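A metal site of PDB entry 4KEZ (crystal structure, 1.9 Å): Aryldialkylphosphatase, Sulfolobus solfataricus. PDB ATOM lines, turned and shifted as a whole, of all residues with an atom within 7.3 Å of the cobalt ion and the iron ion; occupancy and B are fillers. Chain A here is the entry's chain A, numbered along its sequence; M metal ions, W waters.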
ATOM      1  N   HIS A  22      -7.663   5.013  18.545  1.00  0.00           N
ATOM      2  CA  HIS A  22      -8.997   5.383  18.081  1.00  0.00           C
ATOM      3  C   HIS A  22      -9.311   4.743  16.746  1.00  0.00           C
ATOM      4  O   HIS A  22      -9.026   5.316  15.705  1.00  0.00           O
ATOM      5  CB  HIS A  22      -9.126   6.903  17.995  1.00  0.00           C
ATOM      6  CG  HIS A  22     -10.546   7.404  17.839  1.00  0.00           C
ATOM      7  ND1 HIS A  22     -11.050   8.401  18.601  1.00  0.00           N
ATOM      8  CD2 HIS A  22     -11.576   7.006  16.977  1.00  0.00           C
ATOM      9  CE1 HIS A  22     -12.335   8.633  18.249  1.00  0.00           C
ATOM     10  NE2 HIS A  22     -12.655   7.786  17.259  1.00  0.00           N
ATOM     11  N   GLU A  23      -9.889   3.533  16.786  1.00  0.00           N
ATOM     12  CA  GLU A  23     -10.337   2.849  15.563  1.00  0.00           C
ATOM     13  C   GLU A  23     -11.691   2.172  15.832  1.00  0.00           C
ATOM     14  O   GLU A  23     -12.001   1.867  16.977  1.00  0.00           O
ATOM     15  CB  GLU A  23      -9.321   1.794  15.109  1.00  0.00           C
ATOM     16  CG  GLU A  23      -7.861   2.227  15.075  1.00  0.00           C
ATOM     17  CD  GLU A  23      -7.546   3.220  13.976  1.00  0.00           C
ATOM     18  OE1 GLU A  23      -6.489   3.894  14.078  1.00  0.00           O
ATOM     19  OE2 GLU A  23      -8.327   3.328  13.018  1.00  0.00           O
ATOM     20  N   HIS A  24     -12.479   1.946  14.785  1.00  0.00           N
ATOM     21  CA  HIS A  24     -13.802   1.330  14.953  1.00  0.00           C
ATOM     22  C   HIS A  24     -13.907   0.036  14.172  1.00  0.00           C
ATOM     23  O   HIS A  24     -13.745   0.028  12.961  1.00  0.00           O
ATOM     24  CB  HIS A  24     -14.922   2.258  14.472  1.00  0.00           C
ATOM     25  CG  HIS A  24     -15.004   3.573  15.231  1.00  0.00           C
ATOM     26  ND1 HIS A  24     -15.684   3.712  16.386  1.00  0.00           N
ATOM     27  CD2 HIS A  24     -14.485   4.831  14.923  1.00  0.00           C
ATOM     28  CE1 HIS A  24     -15.590   4.982  16.813  1.00  0.00           C
ATOM     29  NE2 HIS A  24     -14.864   5.670  15.911  1.00  0.00           N
ATOM     30  N   VAL A  27     -19.394   0.573  12.808  1.00  0.00           N
ATOM     31  CA  VAL A  27     -20.288   1.628  13.262  1.00  0.00           C
ATOM     32  C   VAL A  27     -21.654   1.475  12.592  1.00  0.00           C
ATOM     33  O   VAL A  27     -21.738   1.219  11.394  1.00  0.00           O
ATOM     34  CB  VAL A  27     -19.705   3.028  12.943  1.00  0.00           C
ATOM     35  CG1 VAL A  27     -20.732   4.125  13.181  1.00  0.00           C
ATOM     36  CG2 VAL A  27     -18.452   3.285  13.768  1.00  0.00           C
ATOM     37  N   ASP A  66     -11.262   0.971  20.886  1.00  0.00           N
ATOM     38  CA  ASP A  66     -12.390   1.165  19.983  1.00  0.00           C
ATOM     39  C   ASP A  66     -13.487   1.948  20.688  1.00  0.00           C
ATOM     40  O   ASP A  66     -14.173   1.420  21.559  1.00  0.00           O
ATOM     41  CB  ASP A  66     -12.923  -0.208  19.522  1.00  0.00           C
ATOM     42  CG  ASP A  66     -14.090  -0.101  18.552  1.00  0.00           C
ATOM     43  OD1 ASP A  66     -14.755   0.962  18.493  1.00  0.00           O
ATOM     44  OD2 ASP A  66     -14.358  -1.102  17.846  1.00  0.00           O
ATOM     45  N   PRO A  67     -13.626   3.244  20.341  1.00  0.00           N
ATOM     46  CA  PRO A  67     -14.567   4.096  21.059  1.00  0.00           C
ATOM     47  C   PRO A  67     -15.987   4.092  20.477  1.00  0.00           C
ATOM     48  O   PRO A  67     -16.696   5.114  20.526  1.00  0.00           O
ATOM     49  CB  PRO A  67     -13.950   5.490  20.915  1.00  0.00           C
ATOM     50  CG  PRO A  67     -13.206   5.442  19.624  1.00  0.00           C
ATOM     51  CD  PRO A  67     -12.756   4.012  19.437  1.00  0.00           C
ATOM     52  N   THR A  68     -16.401   2.943  19.943  1.00  0.00           N
ATOM     53  CA  THR A  68     -17.798   2.739  19.545  1.00  0.00           C
ATOM     54  C   THR A  68     -18.645   2.574  20.807  1.00  0.00           C
ATOM     55  O   THR A  68     -18.458   1.616  21.573  1.00  0.00           O
ATOM     56  CB  THR A  68     -17.936   1.464  18.680  1.00  0.00           C
ATOM     57  OG1 THR A  68     -16.968   1.499  17.628  1.00  0.00           O
ATOM     58  CG2 THR A  68     -19.329   1.369  18.081  1.00  0.00           C
ATOM     59  N   LEU A  72     -23.261   4.851  18.230  1.00  0.00           N
ATOM     60  CA  LEU A  72     -22.404   4.366  17.152  1.00  0.00           C
ATOM     61  C   LEU A  72     -22.535   2.856  16.954  1.00  0.00           C
ATOM     62  O   LEU A  72     -21.828   2.270  16.130  1.00  0.00           O
ATOM     63  CB  LEU A  72     -20.937   4.711  17.416  1.00  0.00           C
ATOM     64  CG  LEU A  72     -20.513   6.178  17.418  1.00  0.00           C
ATOM     65  CD1 LEU A  72     -19.028   6.293  17.719  1.00  0.00           C
ATOM     66  CD2 LEU A  72     -20.841   6.812  16.066  1.00  0.00           C
ATOM     67  N   TYR A  97     -22.641   8.971  22.541  1.00  0.00           N
ATOM     68  CA  TYR A  97     -22.207   9.754  21.408  1.00  0.00           C
ATOM     69  C   TYR A  97     -23.437  10.457  20.836  1.00  0.00           C
ATOM     70  O   TYR A  97     -24.257   9.830  20.160  1.00  0.00           O
ATOM     71  CB  TYR A  97     -21.551   8.829  20.380  1.00  0.00           C
ATOM     72  CG  TYR A  97     -20.957   9.487  19.132  1.00  0.00           C
ATOM     73  CD1 TYR A  97     -21.769   9.901  18.096  1.00  0.00           C
ATOM     74  CD2 TYR A  97     -19.582   9.633  18.987  1.00  0.00           C
ATOM     75  CE1 TYR A  97     -21.236  10.480  16.939  1.00  0.00           C
ATOM     76  CE2 TYR A  97     -19.037  10.214  17.842  1.00  0.00           C
ATOM     77  CZ  TYR A  97     -19.867  10.626  16.824  1.00  0.00           C
ATOM     78  OH  TYR A  97     -19.341  11.191  15.683  1.00  0.00           O
ATOM     79  N   TYR A  99     -24.776  14.622  19.298  1.00  0.00           N
ATOM     80  CA  TYR A  99     -24.373  15.959  18.856  1.00  0.00           C
ATOM     81  C   TYR A  99     -25.340  17.024  19.388  1.00  0.00           C
ATOM     82  O   TYR A  99     -24.962  18.183  19.562  1.00  0.00           O
ATOM     83  CB  TYR A  99     -24.372  16.048  17.335  1.00  0.00           C
ATOM     84  CG  TYR A  99     -23.241  15.317  16.614  1.00  0.00           C
ATOM     85  CD1 TYR A  99     -22.332  14.521  17.296  1.00  0.00           C
ATOM     86  CD2 TYR A  99     -23.121  15.415  15.236  1.00  0.00           C
ATOM     87  CE1 TYR A  99     -21.315  13.859  16.619  1.00  0.00           C
ATOM     88  CE2 TYR A  99     -22.115  14.758  14.553  1.00  0.00           C
ATOM     89  CZ  TYR A  99     -21.216  13.976  15.249  1.00  0.00           C
ATOM     90  OH  TYR A  99     -20.222  13.317  14.554  1.00  0.00           O
ATOM     91  N   KCX A 137     -16.404   7.506  26.507  1.00  0.00           N
ATOM     92  CA  KCX A 137     -16.348   8.290  25.269  1.00  0.00           C
ATOM     93  CB  KCX A 137     -16.480   7.337  24.079  1.00  0.00           C
ATOM     94  CG  KCX A 137     -16.783   8.084  22.780  1.00  0.00           C
ATOM     95  CD  KCX A 137     -15.546   8.795  22.244  1.00  0.00           C
ATOM     96  CE  KCX A 137     -15.837   9.424  20.866  1.00  0.00           C
ATOM     97  NZ  KCX A 137     -15.927   8.427  19.804  1.00  0.00           N
ATOM     98  C   KCX A 137     -17.486   9.273  25.257  1.00  0.00           C
ATOM     99  O   KCX A 137     -18.615   8.916  25.568  1.00  0.00           O
ATOM    100  CX  KCX A 137     -15.611   8.718  18.537  1.00  0.00           C
ATOM    101  OQ1 KCX A 137     -15.719   7.771  17.615  1.00  0.00           O
ATOM    102  OQ2 KCX A 137     -15.215   9.816  18.171  1.00  0.00           O
ATOM    103  N   ILE A 138     -17.183  10.519  24.919  1.00  0.00           N
ATOM    104  CA  ILE A 138     -18.210  11.565  24.789  1.00  0.00           C
ATOM    105  C   ILE A 138     -17.937  12.356  23.511  1.00  0.00           C
ATOM    106  O   ILE A 138     -16.846  12.286  22.945  1.00  0.00           O
ATOM    107  CB  ILE A 138     -18.223  12.496  26.019  1.00  0.00           C
ATOM    108  CG1 ILE A 138     -16.914  13.277  26.119  1.00  0.00           C
ATOM    109  CG2 ILE A 138     -18.466  11.716  27.300  1.00  0.00           C
ATOM    110  CD1 ILE A 138     -16.889  14.554  25.290  1.00  0.00           C
ATOM    111  N   ALA A 139     -18.945  13.105  23.052  1.00  0.00           N
ATOM    112  CA  ALA A 139     -18.825  13.830  21.790  1.00  0.00           C
ATOM    113  C   ALA A 139     -19.444  15.217  21.814  1.00  0.00           C
ATOM    114  O   ALA A 139     -20.325  15.511  22.624  1.00  0.00           O
ATOM    115  CB  ALA A 139     -19.461  13.017  20.656  1.00  0.00           C
ATOM    116  N   ASP A 141     -20.007  18.286  18.362  1.00  0.00           N
ATOM    117  CA  ASP A 141     -19.592  18.590  17.004  1.00  0.00           C
ATOM    118  C   ASP A 141     -20.110  19.968  16.610  1.00  0.00           C
ATOM    119  O   ASP A 141     -20.105  20.897  17.417  1.00  0.00           O
ATOM    120  CB  ASP A 141     -20.065  17.485  16.038  1.00  0.00           C
ATOM    121  CG  ASP A 141     -19.201  17.395  14.778  1.00  0.00           C
ATOM    122  OD1 ASP A 141     -19.302  18.284  13.908  1.00  0.00           O
ATOM    123  OD2 ASP A 141     -18.436  16.410  14.642  1.00  0.00           O
ATOM    124  N   THR A 169     -12.598  11.851  23.726  1.00  0.00           N
ATOM    125  CA  THR A 169     -13.648  12.673  23.152  1.00  0.00           C
ATOM    126  C   THR A 169     -13.631  12.708  21.633  1.00  0.00           C
ATOM    127  O   THR A 169     -12.608  12.441  21.004  1.00  0.00           O
ATOM    128  CB  THR A 169     -13.613  14.121  23.665  1.00  0.00           C
ATOM    129  OG1 THR A 169     -12.699  14.894  22.877  1.00  0.00           O
ATOM    130  CG2 THR A 169     -13.190  14.169  25.133  1.00  0.00           C
ATOM    131  N   HIS A 170     -14.795  13.021  21.097  1.00  0.00           N
ATOM    132  CA  HIS A 170     -14.990  13.403  19.713  1.00  0.00           C
ATOM    133  C   HIS A 170     -15.247  14.868  19.767  1.00  0.00           C
ATOM    134  O   HIS A 170     -16.077  15.324  20.558  1.00  0.00           O
ATOM    135  CB  HIS A 170     -16.231  12.702  19.170  1.00  0.00           C
ATOM    136  CG  HIS A 170     -16.655  13.167  17.800  1.00  0.00           C
ATOM    137  ND1 HIS A 170     -16.493  12.417  16.695  1.00  0.00           N
ATOM    138  CD2 HIS A 170     -17.288  14.345  17.377  1.00  0.00           C
ATOM    139  CE1 HIS A 170     -16.982  13.078  15.617  1.00  0.00           C
ATOM    140  NE2 HIS A 170     -17.458  14.263  16.040  1.00  0.00           N
ATOM    141  N   SER A 171     -14.529  15.639  18.952  1.00  0.00           N
ATOM    142  CA  SER A 171     -14.811  17.070  18.862  1.00  0.00           C
ATOM    143  C   SER A 171     -14.759  17.526  17.407  1.00  0.00           C
ATOM    144  O   SER A 171     -14.365  16.759  16.519  1.00  0.00           O
ATOM    145  CB  SER A 171     -13.847  17.896  19.720  1.00  0.00           C
ATOM    146  OG  SER A 171     -12.623  18.162  19.041  1.00  0.00           O
ATOM    147  N   GLY A 198     -10.329  14.679  21.006  1.00  0.00           N
ATOM    148  CA  GLY A 198     -10.270  14.013  19.715  1.00  0.00           C
ATOM    149  C   GLY A 198     -10.416  14.911  18.500  1.00  0.00           C
ATOM    150  O   GLY A 198     -11.016  15.974  18.561  1.00  0.00           O
ATOM    151  N   HIS A 199      -9.828  14.451  17.394  1.00  0.00           N
ATOM    152  CA  HIS A 199     -10.028  15.043  16.059  1.00  0.00           C
ATOM    153  C   HIS A 199      -9.391  16.379  15.874  1.00  0.00           C
ATOM    154  O   HIS A 199      -9.748  17.137  14.959  1.00  0.00           O
ATOM    155  CB  HIS A 199     -11.513  15.030  15.686  1.00  0.00           C
ATOM    156  CG  HIS A 199     -12.177  13.693  15.902  1.00  0.00           C
ATOM    157  ND1 HIS A 199     -11.500  12.530  15.804  1.00  0.00           N
ATOM    158  CD2 HIS A 199     -13.489  13.352  16.226  1.00  0.00           C
ATOM    159  CE1 HIS A 199     -12.335  11.495  16.038  1.00  0.00           C
ATOM    160  NE2 HIS A 199     -13.551  12.002  16.300  1.00  0.00           N
ATOM    161  N   ASP A 222      -5.899  12.063  14.920  1.00  0.00           N
ATOM    162  CA  ASP A 222      -6.461  10.720  14.975  1.00  0.00           C
ATOM    163  C   ASP A 222      -7.361  10.345  13.796  1.00  0.00           C
ATOM    164  O   ASP A 222      -8.100   9.376  13.879  1.00  0.00           O
ATOM    165  CB  ASP A 222      -7.245  10.570  16.264  1.00  0.00           C
ATOM    166  CG  ASP A 222      -8.328  11.628  16.426  1.00  0.00           C
ATOM    167  OD1 ASP A 222      -8.725  12.261  15.410  1.00  0.00           O
ATOM    168  OD2 ASP A 222      -8.784  11.842  17.570  1.00  0.00           O
ATOM    169  N   ARG A 223      -7.293  11.104  12.709  1.00  0.00           N
ATOM    170  CA  ARG A 223      -8.139  10.814  11.553  1.00  0.00           C
ATOM    171  C   ARG A 223      -7.351  10.714  10.246  1.00  0.00           C
ATOM    172  O   ARG A 223      -7.821  11.099   9.166  1.00  0.00           O
ATOM    173  CB  ARG A 223      -9.291  11.826  11.447  1.00  0.00           C
ATOM    174  CG  ARG A 223     -10.435  11.515  12.406  1.00  0.00           C
ATOM    175  CD  ARG A 223     -11.515  12.597  12.373  1.00  0.00           C
ATOM    176  NE  ARG A 223     -12.854  12.049  12.630  1.00  0.00           N
ATOM    177  CZ  ARG A 223     -13.945  12.794  12.709  1.00  0.00           C
ATOM    178  NH1 ARG A 223     -13.867  14.113  12.578  1.00  0.00           N
ATOM    179  NH2 ARG A 223     -15.136  12.231  12.921  1.00  0.00           N
ATOM    180  N   HIS A 255      -6.373   6.565  13.032  1.00  0.00           N
ATOM    181  CA  HIS A 255      -7.063   6.777  11.755  1.00  0.00           C
ATOM    182  C   HIS A 255      -8.530   7.021  11.896  1.00  0.00           C
ATOM    183  O   HIS A 255      -9.157   7.548  10.973  1.00  0.00           O
ATOM    184  CB  HIS A 255      -6.911   5.574  10.837  1.00  0.00           C
ATOM    185  CG  HIS A 255      -5.502   5.049  10.732  1.00  0.00           C
ATOM    186  ND1 HIS A 255      -5.014   4.093  11.554  1.00  0.00           N
ATOM    187  CD2 HIS A 255      -4.481   5.349   9.831  1.00  0.00           C
ATOM    188  CE1 HIS A 255      -3.742   3.808  11.204  1.00  0.00           C
ATOM    189  NE2 HIS A 255      -3.418   4.584  10.157  1.00  0.00           N
ATOM    190  N   ASP A 256      -9.105   6.621  13.030  1.00  0.00           N
ATOM    191  CA  ASP A 256     -10.566   6.653  13.200  1.00  0.00           C
ATOM    192  C   ASP A 256     -11.194   5.760  12.143  1.00  0.00           C
ATOM    193  O   ASP A 256     -12.313   6.003  11.671  1.00  0.00           O
ATOM    194  CB  ASP A 256     -11.100   8.095  13.053  1.00  0.00           C
ATOM    195  CG  ASP A 256     -12.516   8.263  13.615  1.00  0.00           C
ATOM    196  OD1 ASP A 256     -12.990   7.379  14.345  1.00  0.00           O
ATOM    197  OD2 ASP A 256     -13.148   9.316  13.337  1.00  0.00           O
ATOM    198  N   TYR A 257     -10.468   4.725  11.743  1.00  0.00           N
ATOM    199  CA  TYR A 257     -10.947   3.910  10.641  1.00  0.00           C
ATOM    200  C   TYR A 257     -12.159   3.078  11.026  1.00  0.00           C
ATOM    201  O   TYR A 257     -12.182   2.437  12.085  1.00  0.00           O
ATOM    202  CB  TYR A 257      -9.852   3.013  10.066  1.00  0.00           C
ATOM    203  CG  TYR A 257     -10.327   2.345   8.795  1.00  0.00           C
ATOM    204  CD1 TYR A 257     -10.531   3.098   7.641  1.00  0.00           C
ATOM    205  CD2 TYR A 257     -10.605   0.985   8.760  1.00  0.00           C
ATOM    206  CE1 TYR A 257     -10.990   2.495   6.477  1.00  0.00           C
ATOM    207  CE2 TYR A 257     -11.062   0.384   7.611  1.00  0.00           C
ATOM    208  CZ  TYR A 257     -11.255   1.139   6.469  1.00  0.00           C
ATOM    209  OH  TYR A 257     -11.710   0.531   5.327  1.00  0.00           O
ATOM    210  N   CYS A 258     -13.171   3.089  10.167  1.00  0.00           N
ATOM    211  CA  CYS A 258     -14.345   2.264  10.376  1.00  0.00           C
ATOM    212  C   CYS A 258     -14.349   1.103   9.380  1.00  0.00           C
ATOM    213  O   CYS A 258     -14.523   1.321   8.184  1.00  0.00           O
ATOM    214  CB  CYS A 258     -15.617   3.102  10.226  1.00  0.00           C
ATOM    215  SG  CYS A 258     -15.679   4.534  11.324  1.00  0.00           S
HETATM  216 CO    CO M   1     -15.173  10.837  16.538  1.00  0.00          CO
HETATM  217 FE    FE M   2     -14.378   7.625  16.083  1.00  0.00          FE
HETATM  218  O   HOH W   1     -17.411   9.552  14.280  1.00  0.00           O
HETATM  219  O   HOH W   2     -14.950   9.283  15.245  1.00  0.00           O
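Of the 25 residues printed, 4 come within 4 Å of the iron ion.
NZ of KCX 137 is in hydrogen-bond range of the backbone carbonyl oxygen (O) of Pro 67, 3.5 Å away.
A ring nitrogen (ND1) of His 199 sits close to the guanidinium group (NE) of Arg 223 (3.5 Å).
A ring nitrogen (ND1) of His 199 lies within hydrogen-bond range of the side-chain carboxylate (OD1) of Asp 222, at 2.8 Å.
The backbone carbonyl oxygen of Tyr 257 is in hydrogen-bond range of the backbone NH of His 24 (2.8 Å).
A ring nitrogen (NE2) of His 170 is in hydrogen-bond range of the side-chain hydroxyl (OH) of Tyr 99, 3.3 Å away.
The backbone NH (N) of His 170 is in hydrogen-bond range of the backbone carbonyl oxygen (O) of Ile 138 (2.9 Å).
The backbone carbonyl oxygen of Asp 256 lies within hydrogen-bond range of the side-chain sulfur of Cys 258, 3.7 Å away.
The side-chain carboxylate (OE2) of Glu 23 lies within hydrogen-bond range of the backbone NH (N) of Asp 256 (3.4 Å).
Residues that only touch the cobalt ion: Arg 223.
Along chain A the residues within 4 Å of the cobalt ion span positions 22 to 223.
The nearest printed residue that does not touch the cobalt ion is Asp 256 (4.1 Å).
OQ2 of KCX 137 is bound to the cobalt ion (1.9 Å).
NE2 of His 199 binds the cobalt ion, 2.0 Å away.
The cobalt ion is bound by water W2 (2.0 Å).
A ring nitrogen (ND1) of His 170 binds the cobalt ion.
The cobalt ion has four donor atoms within binding distance.
The iron ion is bound by water W2 (1.9 Å), a ring nitrogen (NE2) of His 24 (2.0 Å), OQ1 of KCX 137 (2.0 Å), a ring nitrogen (NE2) of His 22 (2.1 Å) and the side-chain carboxylate of Asp 256 (2.2 Å).
The iron ion has five donor atoms within binding distance.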
